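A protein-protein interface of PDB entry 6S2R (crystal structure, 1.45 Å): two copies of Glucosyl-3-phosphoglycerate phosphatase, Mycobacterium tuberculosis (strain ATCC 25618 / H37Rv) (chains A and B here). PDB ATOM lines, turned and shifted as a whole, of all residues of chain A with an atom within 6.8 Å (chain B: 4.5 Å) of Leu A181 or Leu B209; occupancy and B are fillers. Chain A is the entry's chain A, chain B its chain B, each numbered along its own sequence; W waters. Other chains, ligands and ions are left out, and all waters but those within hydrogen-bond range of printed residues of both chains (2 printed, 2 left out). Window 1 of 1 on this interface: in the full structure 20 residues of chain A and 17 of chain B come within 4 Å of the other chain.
The backbone NH (N) of Leu B209 lies within hydrogen-bond range of the backbone carbonyl oxygen (O) of Ala A180 (2.7 Å). N of Gly A182 lies within hydrogen-bond range of O of Leu B209, at 3.0 Å. The indole nitrogen of Trp A212 sits close to the backbone carbonyl oxygen of Asp B210 (3.3 Å). O of Trp A212 sits at hydrogen-bond distance from N of Trp B212. ND2 of Asn A213 lies within hydrogen-bond range of O of Asp B210.
O of Gly A183 is in hydrogen-bond range of NE1 of Trp A212, 3.3 Å away. ND2 of Asn A213 is in hydrogen-bond range of O of Gly A183 (3.5 Å). O of Gln B191 sits at hydrogen-bond distance from N of Asp B210 (2.8 Å). N of Gln B191 lies within hydrogen-bond range of O of Val B211. The side-chain carboxylate of Asp B210 lies within salt-bridge range of the guanidinium group of Arg B208.
Pro A179 touches Arg B208. O of Ala A180 touches C of Arg B208, at 3.7 Å. CD2 of Leu A181 touches CD2 of Leu B209, 3.8 Å away. Gly A183 touches Arg B208. Asp B210 touches Gly A183 (O to O, 3.8 Å). O of Leu A209 touches C of Leu B181, at 3.9 Å. Leu A209 touches Trp B212. O of Leu B209 touches NE1 of Trp A212, 3.5 Å away. Trp A212 touches Val B211 (O to CA, 3.3 Å). O of Asn A213 touches CG2 of Val B211 (3.9 Å).
Of the printed residues of chain B, Gly A182 touches Arg B208 and Leu B209. Of the printed residues of chain B, Leu A209 touches Leu B181 (3.9 Å) and Trp B212 (3.8 Å). Printed residues of chain B within 4 Å of Asn A213: Asp B210 and Val B211. Leu B171 touches none of the printed residues of chain A. Of the printed residues of chain A, Leu B209 touches Ala A180, Leu A181, Gly A182 and Trp A212. Of the printed residues of chain A, Asp B210 touches Gly A183, Trp A212 and Asn A213. Printed residues of chain A within 4 Å of Val B211: Trp A212 (3.3 Å) and Asn A213 (3.9 Å). The nearest printed residue of chain A that does not touch Leu B209 is Leu A209 (4.02 Å). The nearest printed residue of chain A that does not touch Trp B212 is Asn A213 (5.0 Å).
Of the 10 printed residues of chain B, 6 touch a printed residue of chain A. Among the printed residues, no Asp or Glu carboxylate lies within 4 Å of a Lys or Arg side-chain nitrogen of the other chain.
Leu A181 touches Leu B209, and with the chains exchanged Leu A209 touches Leu B181. Leu A209 touches Trp B212, and with the chains exchanged Trp A212 touches Leu B209. Trp A212 touches its own counterpart, Trp B212. Positions printed for both chains: 171, 181, 209 and 212. Of the 17 pairs that touch across the chains among the printed residues, 5 have their exchanged pair printed and touching as well.
Water W2 bridges the backbone carbonyl oxygen (O) of Leu B171 (2.7 Å) and the side-chain amide oxygen (OD1) of Asn A177 (2.9 Å). Water W1 lies within hydrogen-bond range of the guanidinium group of Arg A110 and the guanidinium group of Arg B208.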
ATOM      1  N   ARG A 110      -1.746  11.308 -18.913  1.00  0.00           N
ATOM      2  CA  ARG A 110      -0.642  12.266 -18.942  1.00  0.00           C
ATOM      3  C   ARG A 110      -0.924  13.455 -19.857  1.00  0.00           C
ATOM      4  O   ARG A 110      -0.351  14.532 -19.668  1.00  0.00           O
ATOM      5  CB  ARG A 110       0.634  11.560 -19.409  1.00  0.00           C
ATOM      6  CG  ARG A 110       1.316  10.790 -18.296  1.00  0.00           C
ATOM      7  CD  ARG A 110       2.335  11.666 -17.580  1.00  0.00           C
ATOM      8  NE  ARG A 110       2.874  11.037 -16.372  1.00  0.00           N
ATOM      9  CZ  ARG A 110       2.707  11.508 -15.139  1.00  0.00           C
ATOM     10  NH1 ARG A 110       2.030  12.630 -14.934  1.00  0.00           N
ATOM     11  NH2 ARG A 110       3.230  10.860 -14.107  1.00  0.00           N
ATOM     12  N   ARG A 123      -7.011  15.948 -12.494  1.00  0.00           N
ATOM     13  CA  ARG A 123      -6.217  17.057 -11.985  1.00  0.00           C
ATOM     14  C   ARG A 123      -7.069  18.304 -11.764  1.00  0.00           C
ATOM     15  O   ARG A 123      -6.805  19.085 -10.839  1.00  0.00           O
ATOM     16  CB  ARG A 123      -5.010  17.294 -12.896  1.00  0.00           C
ATOM     17  CG  ARG A 123      -4.041  16.077 -12.943  1.00  0.00           C
ATOM     18  CD  ARG A 123      -3.205  15.946 -11.645  1.00  0.00           C
ATOM     19  NE  ARG A 123      -2.211  14.860 -11.679  1.00  0.00           N
ATOM     20  CZ  ARG A 123      -1.030  14.928 -12.293  1.00  0.00           C
ATOM     21  NH1 ARG A 123      -0.668  16.032 -12.940  1.00  0.00           N
ATOM     22  NH2 ARG A 123      -0.186  13.909 -12.237  1.00  0.00           N
ATOM     23  N   ILE A 163       0.891  19.191  -6.967  1.00  0.00           N
ATOM     24  CA  ILE A 163       1.702  20.372  -7.253  1.00  0.00           C
ATOM     25  C   ILE A 163       1.517  20.835  -8.698  1.00  0.00           C
ATOM     26  O   ILE A 163       1.410  22.039  -8.959  1.00  0.00           O
ATOM     27  CB  ILE A 163       3.172  20.132  -6.887  1.00  0.00           C
ATOM     28  CG1 ILE A 163       3.280  20.032  -5.365  1.00  0.00           C
ATOM     29  CG2 ILE A 163       4.061  21.282  -7.411  1.00  0.00           C
ATOM     30  CD1 ILE A 163       4.638  19.545  -4.865  1.00  0.00           C
ATOM     31  N   ALA A 164       1.459  19.892  -9.647  1.00  0.00           N
ATOM     32  CA  ALA A 164       1.224  20.268 -11.043  1.00  0.00           C
ATOM     33  C   ALA A 164      -0.157  20.892 -11.239  1.00  0.00           C
ATOM     34  O   ALA A 164      -0.303  21.909 -11.925  1.00  0.00           O
ATOM     35  CB  ALA A 164       1.338  19.029 -11.942  1.00  0.00           C
ATOM     36  N   ALA A 165      -1.181  20.324 -10.607  1.00  0.00           N
ATOM     37  CA  ALA A 165      -2.542  20.814 -10.813  1.00  0.00           C
ATOM     38  C   ALA A 165      -2.717  22.186 -10.165  1.00  0.00           C
ATOM     39  O   ALA A 165      -3.240  23.140 -10.773  1.00  0.00           O
ATOM     40  CB  ALA A 165      -3.536  19.804 -10.208  1.00  0.00           C
ATOM     41  N   LEU A 166      -2.282  22.298  -8.910  1.00  0.00           N
ATOM     42  CA  LEU A 166      -2.420  23.562  -8.210  1.00  0.00           C
ATOM     43  C   LEU A 166      -1.599  24.660  -8.877  1.00  0.00           C
ATOM     44  O   LEU A 166      -2.066  25.800  -9.005  1.00  0.00           O
ATOM     45  CB  LEU A 166      -2.049  23.361  -6.735  1.00  0.00           C
ATOM     46  CG  LEU A 166      -2.137  24.626  -5.885  1.00  0.00           C
ATOM     47  CD1 LEU A 166      -3.543  25.221  -5.908  1.00  0.00           C
ATOM     48  CD2 LEU A 166      -1.765  24.280  -4.456  1.00  0.00           C
ATOM     49  N   SER A 167      -0.379  24.343  -9.335  1.00  0.00           N
ATOM     50  CA  SER A 167       0.410  25.368  -9.998  1.00  0.00           C
ATOM     51  C   SER A 167      -0.260  25.850 -11.279  1.00  0.00           C
ATOM     52  O   SER A 167      -0.342  27.058 -11.526  1.00  0.00           O
ATOM     53  CB  SER A 167       1.811  24.832 -10.338  1.00  0.00           C
ATOM     54  OG  SER A 167       2.565  24.568  -9.157  1.00  0.00           O
ATOM     55  N   ALA A 168      -0.715  24.911 -12.122  1.00  0.00           N
ATOM     56  CA  ALA A 168      -1.375  25.308 -13.359  1.00  0.00           C
ATOM     57  C   ALA A 168      -2.604  26.166 -13.087  1.00  0.00           C
ATOM     58  O   ALA A 168      -2.874  27.133 -13.813  1.00  0.00           O
ATOM     59  CB  ALA A 168      -1.808  24.054 -14.114  1.00  0.00           C
ATOM     60  N   ALA A 169      -3.362  25.844 -12.020  1.00  0.00           N
ATOM     61  CA  ALA A 169      -4.561  26.624 -11.691  1.00  0.00           C
ATOM     62  C   ALA A 169      -4.206  28.036 -11.219  1.00  0.00           C
ATOM     63  O   ALA A 169      -4.887  29.011 -11.565  1.00  0.00           O
ATOM     64  CB  ALA A 169      -5.437  25.914 -10.629  1.00  0.00           C
ATOM     65  N   LEU A 171      -1.521  29.747 -12.026  1.00  0.00           N
ATOM     66  CA  LEU A 171      -1.092  30.426 -13.245  1.00  0.00           C
ATOM     67  C   LEU A 171      -2.254  30.744 -14.177  1.00  0.00           C
ATOM     68  O   LEU A 171      -2.061  31.526 -15.111  1.00  0.00           O
ATOM     69  CB  LEU A 171      -0.075  29.551 -13.990  1.00  0.00           C
ATOM     70  CG  LEU A 171       1.206  29.272 -13.211  1.00  0.00           C
ATOM     71  CD1 LEU A 171       2.047  28.204 -13.940  1.00  0.00           C
ATOM     72  CD2 LEU A 171       2.004  30.542 -13.030  1.00  0.00           C
ATOM     73  N   LEU A 173      -3.487  28.858 -16.367  1.00  0.00           N
ATOM     74  CA  LEU A 173      -3.394  28.230 -17.680  1.00  0.00           C
ATOM     75  C   LEU A 173      -4.752  27.638 -18.024  1.00  0.00           C
ATOM     76  O   LEU A 173      -5.448  27.142 -17.131  1.00  0.00           O
ATOM     77  CB  LEU A 173      -2.383  27.078 -17.640  1.00  0.00           C
ATOM     78  CG  LEU A 173      -0.932  27.469 -17.397  1.00  0.00           C
ATOM     79  CD1 LEU A 173      -0.074  26.221 -17.325  1.00  0.00           C
ATOM     80  CD2 LEU A 173      -0.494  28.391 -18.530  1.00  0.00           C
ATOM     81  N   ASN A 177      -3.987  23.063 -21.365  1.00  0.00           N
ATOM     82  CA  ASN A 177      -2.542  23.217 -21.311  1.00  0.00           C
ATOM     83  C   ASN A 177      -1.956  22.805 -19.981  1.00  0.00           C
ATOM     84  O   ASN A 177      -0.734  22.883 -19.810  1.00  0.00           O
ATOM     85  CB  ASN A 177      -2.177  24.662 -21.625  1.00  0.00           C
ATOM     86  CG  ASN A 177      -2.703  25.081 -22.971  1.00  0.00           C
ATOM     87  OD1 ASN A 177      -2.174  24.680 -24.019  1.00  0.00           O
ATOM     88  ND2 ASN A 177      -3.741  25.844 -22.958  1.00  0.00           N
ATOM     89  N   TRP A 178      -2.784  22.385 -19.027  1.00  0.00           N
ATOM     90  CA  TRP A 178      -2.217  21.884 -17.776  1.00  0.00           C
ATOM     91  C   TRP A 178      -1.210  20.746 -17.944  1.00  0.00           C
ATOM     92  O   TRP A 178      -0.264  20.684 -17.139  1.00  0.00           O
ATOM     93  CB  TRP A 178      -3.324  21.476 -16.805  1.00  0.00           C
ATOM     94  CG  TRP A 178      -4.117  22.600 -16.242  1.00  0.00           C
ATOM     95  CD1 TRP A 178      -4.172  23.881 -16.698  1.00  0.00           C
ATOM     96  CD2 TRP A 178      -4.945  22.549 -15.057  1.00  0.00           C
ATOM     97  NE1 TRP A 178      -5.039  24.617 -15.917  1.00  0.00           N
ATOM     98  CE2 TRP A 178      -5.493  23.833 -14.887  1.00  0.00           C
ATOM     99  CE3 TRP A 178      -5.270  21.539 -14.156  1.00  0.00           C
ATOM    100  CZ2 TRP A 178      -6.392  24.131 -13.863  1.00  0.00           C
ATOM    101  CZ3 TRP A 178      -6.129  21.847 -13.114  1.00  0.00           C
ATOM    102  CH2 TRP A 178      -6.679  23.130 -12.985  1.00  0.00           C
ATOM    103  N   PRO A 179      -1.354  19.812 -18.891  1.00  0.00           N
ATOM    104  CA  PRO A 179      -0.361  18.740 -19.031  1.00  0.00           C
ATOM    105  C   PRO A 179       1.024  19.249 -19.403  1.00  0.00           C
ATOM    106  O   PRO A 179       1.967  18.450 -19.413  1.00  0.00           O
ATOM    107  CB  PRO A 179      -0.950  17.849 -20.142  1.00  0.00           C
ATOM    108  CG  PRO A 179      -2.438  18.073 -19.999  1.00  0.00           C
ATOM    109  CD  PRO A 179      -2.549  19.542 -19.717  1.00  0.00           C
ATOM    110  N   ALA A 180       1.164  20.539 -19.730  1.00  0.00           N
ATOM    111  CA  ALA A 180       2.513  21.076 -19.938  1.00  0.00           C
ATOM    112  C   ALA A 180       3.392  20.934 -18.711  1.00  0.00           C
ATOM    113  O   ALA A 180       4.617  20.941 -18.869  1.00  0.00           O
ATOM    114  CB  ALA A 180       2.471  22.556 -20.370  1.00  0.00           C
ATOM    115  N   LEU A 181       2.824  20.820 -17.504  1.00  0.00           N
ATOM    116  CA  LEU A 181       3.617  20.718 -16.277  1.00  0.00           C
ATOM    117  C   LEU A 181       3.678  19.270 -15.841  1.00  0.00           C
ATOM    118  O   LEU A 181       2.641  18.600 -15.745  1.00  0.00           O
ATOM    119  CB  LEU A 181       3.004  21.538 -15.138  1.00  0.00           C
ATOM    120  CG  LEU A 181       2.912  23.046 -15.323  1.00  0.00           C
ATOM    121  CD1 LEU A 181       2.342  23.662 -14.039  1.00  0.00           C
ATOM    122  CD2 LEU A 181       4.256  23.668 -15.669  1.00  0.00           C
ATOM    123  N   GLY A 182       4.906  18.759 -15.812  1.00  0.00           N
ATOM    124  CA  GLY A 182       5.183  17.356 -15.772  1.00  0.00           C
ATOM    125  C   GLY A 182       5.319  16.874 -14.358  1.00  0.00           C
ATOM    126  O   GLY A 182       4.560  17.286 -13.471  1.00  0.00           O
ATOM    127  N   GLY A 183       6.267  15.995 -14.158  1.00  0.00           N
ATOM    128  CA  GLY A 183       6.496  15.426 -12.864  1.00  0.00           C
ATOM    129  C   GLY A 183       7.354  16.304 -11.996  1.00  0.00           C
ATOM    130  O   GLY A 183       7.985  17.281 -12.413  1.00  0.00           O
ATOM    131  N   LEU A 209       5.477  31.452 -12.722  1.00  0.00           N
ATOM    132  CA  LEU A 209       6.241  30.259 -12.366  1.00  0.00           C
ATOM    133  C   LEU A 209       7.718  30.642 -12.283  1.00  0.00           C
ATOM    134  O   LEU A 209       8.377  30.845 -13.302  1.00  0.00           O
ATOM    135  CB  LEU A 209       6.011  29.145 -13.389  1.00  0.00           C
ATOM    136  CG  LEU A 209       6.745  27.816 -13.189  1.00  0.00           C
ATOM    137  CD1 LEU A 209       6.384  27.170 -11.888  1.00  0.00           C
ATOM    138  CD2 LEU A 209       6.443  26.854 -14.365  1.00  0.00           C
ATOM    139  N   TRP A 212      10.322  25.411 -11.489  1.00  0.00           N
ATOM    140  CA  TRP A 212       9.578  24.155 -11.491  1.00  0.00           C
ATOM    141  C   TRP A 212      10.557  23.019 -11.280  1.00  0.00           C
ATOM    142  O   TRP A 212      11.470  22.848 -12.070  1.00  0.00           O
ATOM    143  CB  TRP A 212       8.802  23.943 -12.818  1.00  0.00           C
ATOM    144  CG  TRP A 212       8.144  22.594 -12.902  1.00  0.00           C
ATOM    145  CD1 TRP A 212       8.616  21.487 -13.522  1.00  0.00           C
ATOM    146  CD2 TRP A 212       6.910  22.204 -12.257  1.00  0.00           C
ATOM    147  NE1 TRP A 212       7.759  20.427 -13.325  1.00  0.00           N
ATOM    148  CE2 TRP A 212       6.720  20.842 -12.526  1.00  0.00           C
ATOM    149  CE3 TRP A 212       5.974  22.885 -11.468  1.00  0.00           C
ATOM    150  CZ2 TRP A 212       5.594  20.130 -12.082  1.00  0.00           C
ATOM    151  CZ3 TRP A 212       4.869  22.171 -10.973  1.00  0.00           C
ATOM    152  CH2 TRP A 212       4.696  20.815 -11.290  1.00  0.00           C
ATOM    153  N   ASN A 213      10.383  22.245 -10.219  1.00  0.00           N
ATOM    154  CA  ASN A 213      11.073  20.973 -10.023  1.00  0.00           C
ATOM    155  C   ASN A 213      12.592  21.133  -9.866  1.00  0.00           C
ATOM    156  O   ASN A 213      13.383  20.441 -10.517  1.00  0.00           O
ATOM    157  CB  ASN A 213      10.697  19.965 -11.115  1.00  0.00           C
ATOM    158  CG  ASN A 213      11.149  18.559 -10.807  1.00  0.00           C
ATOM    159  OD1 ASN A 213      11.202  18.148  -9.656  1.00  0.00           O
ATOM    160  ND2 ASN A 213      11.396  17.776 -11.838  1.00  0.00           N
ATOM    161  N   LEU B 171       6.052  23.653 -25.949  1.00  0.00           N
ATOM    162  CA  LEU B 171       4.927  23.218 -25.113  1.00  0.00           C
ATOM    163  C   LEU B 171       3.570  23.531 -25.718  1.00  0.00           C
ATOM    164  O   LEU B 171       2.552  23.014 -25.230  1.00  0.00           O
ATOM    165  CB  LEU B 171       5.052  23.894 -23.749  1.00  0.00           C
ATOM    166  CG  LEU B 171       6.291  23.538 -22.916  1.00  0.00           C
ATOM    167  CD1 LEU B 171       6.448  24.520 -21.730  1.00  0.00           C
ATOM    168  CD2 LEU B 171       6.264  22.081 -22.425  1.00  0.00           C
ATOM    169  N   LEU B 181       5.983  31.906 -17.608  1.00  0.00           N
ATOM    170  CA  LEU B 181       7.346  31.461 -17.302  1.00  0.00           C
ATOM    171  C   LEU B 181       8.163  32.643 -16.785  1.00  0.00           C
ATOM    172  O   LEU B 181       8.404  33.607 -17.518  1.00  0.00           O
ATOM    173  CB  LEU B 181       8.000  30.859 -18.550  1.00  0.00           C
ATOM    174  CG  LEU B 181       7.295  29.633 -19.144  1.00  0.00           C
ATOM    175  CD1 LEU B 181       7.957  29.079 -20.399  1.00  0.00           C
ATOM    176  CD2 LEU B 181       7.145  28.502 -18.086  1.00  0.00           C
ATOM    177  N   THR B 190      16.721  24.402 -17.699  1.00  0.00           N
ATOM    178  CA  THR B 190      15.364  23.966 -17.950  1.00  0.00           C
ATOM    179  C   THR B 190      15.422  22.649 -18.687  1.00  0.00           C
ATOM    180  O   THR B 190      16.382  22.380 -19.412  1.00  0.00           O
ATOM    181  CB  THR B 190      14.662  25.077 -18.734  1.00  0.00           C
ATOM    182  OG1 THR B 190      14.234  26.083 -17.789  1.00  0.00           O
ATOM    183  CG2 THR B 190      13.438  24.634 -19.572  1.00  0.00           C
ATOM    184  N   GLN B 191      14.438  21.792 -18.464  1.00  0.00           N
ATOM    185  CA  GLN B 191      14.414  20.530 -19.184  1.00  0.00           C
ATOM    186  C   GLN B 191      12.994  20.281 -19.672  1.00  0.00           C
ATOM    187  O   GLN B 191      12.030  20.407 -18.911  1.00  0.00           O
ATOM    188  CB  GLN B 191      14.867  19.355 -18.334  1.00  0.00           C
ATOM    189  CG  GLN B 191      14.801  18.007 -19.082  1.00  0.00           C
ATOM    190  CD  GLN B 191      15.336  16.868 -18.245  1.00  0.00           C
ATOM    191  OE1 GLN B 191      16.489  16.925 -17.765  1.00  0.00           O
ATOM    192  NE2 GLN B 191      14.515  15.832 -18.041  1.00  0.00           N
ATOM    193  N   LEU B 192      12.872  19.942 -20.944  1.00  0.00           N
ATOM    194  CA  LEU B 192      11.624  19.484 -21.535  1.00  0.00           C
ATOM    195  C   LEU B 192      11.780  18.036 -21.954  1.00  0.00           C
ATOM    196  O   LEU B 192      12.892  17.582 -22.249  1.00  0.00           O
ATOM    197  CB  LEU B 192      11.250  20.319 -22.770  1.00  0.00           C
ATOM    198  CG  LEU B 192      10.612  21.705 -22.540  1.00  0.00           C
ATOM    199  CD1 LEU B 192      11.456  22.642 -21.737  1.00  0.00           C
ATOM    200  CD2 LEU B 192      10.295  22.365 -23.896  1.00  0.00           C
ATOM    201  N   ARG B 208       6.654  18.284 -22.656  1.00  0.00           N
ATOM    202  CA  ARG B 208       6.211  18.566 -21.297  1.00  0.00           C
ATOM    203  C   ARG B 208       7.390  19.126 -20.521  1.00  0.00           C
ATOM    204  O   ARG B 208       8.543  18.733 -20.753  1.00  0.00           O
ATOM    205  CB  ARG B 208       5.697  17.272 -20.657  1.00  0.00           C
ATOM    206  CG  ARG B 208       5.458  17.281 -19.167  1.00  0.00           C
ATOM    207  CD  ARG B 208       5.062  15.863 -18.764  1.00  0.00           C
ATOM    208  NE  ARG B 208       6.030  15.238 -17.867  1.00  0.00           N
ATOM    209  CZ  ARG B 208       6.103  13.930 -17.636  1.00  0.00           C
ATOM    210  NH1 ARG B 208       7.012  13.453 -16.796  1.00  0.00           N
ATOM    211  NH2 ARG B 208       5.284  13.095 -18.261  1.00  0.00           N
ATOM    212  N   LEU B 209       7.091  20.052 -19.606  1.00  0.00           N
ATOM    213  CA  LEU B 209       8.107  20.752 -18.838  1.00  0.00           C
ATOM    214  C   LEU B 209       8.470  19.880 -17.657  1.00  0.00           C
ATOM    215  O   LEU B 209       7.642  19.654 -16.769  1.00  0.00           O
ATOM    216  CB  LEU B 209       7.605  22.118 -18.376  1.00  0.00           C
ATOM    217  CG  LEU B 209       8.540  23.067 -17.632  1.00  0.00           C
ATOM    218  CD1 LEU B 209       9.658  23.544 -18.571  1.00  0.00           C
ATOM    219  CD2 LEU B 209       7.745  24.282 -17.160  1.00  0.00           C
ATOM    220  N   ASP B 210       9.700  19.376 -17.647  1.00  0.00           N
ATOM    221  CA  ASP B 210      10.208  18.594 -16.531  1.00  0.00           C
ATOM    222  C   ASP B 210      10.831  19.485 -15.457  1.00  0.00           C
ATOM    223  O   ASP B 210      10.670  19.197 -14.269  1.00  0.00           O
ATOM    224  CB  ASP B 210      11.315  17.636 -17.010  1.00  0.00           C
ATOM    225  CG  ASP B 210      10.841  16.600 -18.016  1.00  0.00           C
ATOM    226  OD1 ASP B 210       9.649  16.247 -18.075  1.00  0.00           O
ATOM    227  OD2 ASP B 210      11.727  16.092 -18.748  1.00  0.00           O
ATOM    228  N   VAL B 211      11.567  20.514 -15.852  1.00  0.00           N
ATOM    229  CA  VAL B 211      12.321  21.394 -14.952  1.00  0.00           C
ATOM    230  C   VAL B 211      12.277  22.792 -15.549  1.00  0.00           C
ATOM    231  O   VAL B 211      12.515  22.967 -16.761  1.00  0.00           O
ATOM    232  CB  VAL B 211      13.793  20.924 -14.806  1.00  0.00           C
ATOM    233  CG1 VAL B 211      14.577  21.886 -13.939  1.00  0.00           C
ATOM    234  CG2 VAL B 211      13.895  19.514 -14.251  1.00  0.00           C
ATOM    235  N   TRP B 212      12.006  23.802 -14.729  1.00  0.00           N
ATOM    236  CA  TRP B 212      12.119  25.193 -15.162  1.00  0.00           C
ATOM    237  C   TRP B 212      13.002  25.950 -14.182  1.00  0.00           C
ATOM    238  O   TRP B 212      12.706  26.012 -12.990  1.00  0.00           O
ATOM    239  CB  TRP B 212      10.748  25.889 -15.285  1.00  0.00           C
ATOM    240  CG  TRP B 212      10.915  27.340 -15.687  1.00  0.00           C
ATOM    241  CD1 TRP B 212      10.846  28.425 -14.873  1.00  0.00           C
ATOM    242  CD2 TRP B 212      11.256  27.845 -16.996  1.00  0.00           C
ATOM    243  NE1 TRP B 212      11.094  29.581 -15.596  1.00  0.00           N
ATOM    244  CE2 TRP B 212      11.325  29.245 -16.905  1.00  0.00           C
ATOM    245  CE3 TRP B 212      11.448  27.239 -18.258  1.00  0.00           C
ATOM    246  CZ2 TRP B 212      11.662  30.057 -17.995  1.00  0.00           C
ATOM    247  CZ3 TRP B 212      11.783  28.053 -19.352  1.00  0.00           C
ATOM    248  CH2 TRP B 212      11.883  29.432 -19.211  1.00  0.00           C
HETATM  249  O   HOH W   1       3.161  14.471 -16.532  1.00  0.00           O
HETATM  250  O   HOH W   2       0.263  23.083 -23.840  1.00  0.00           O
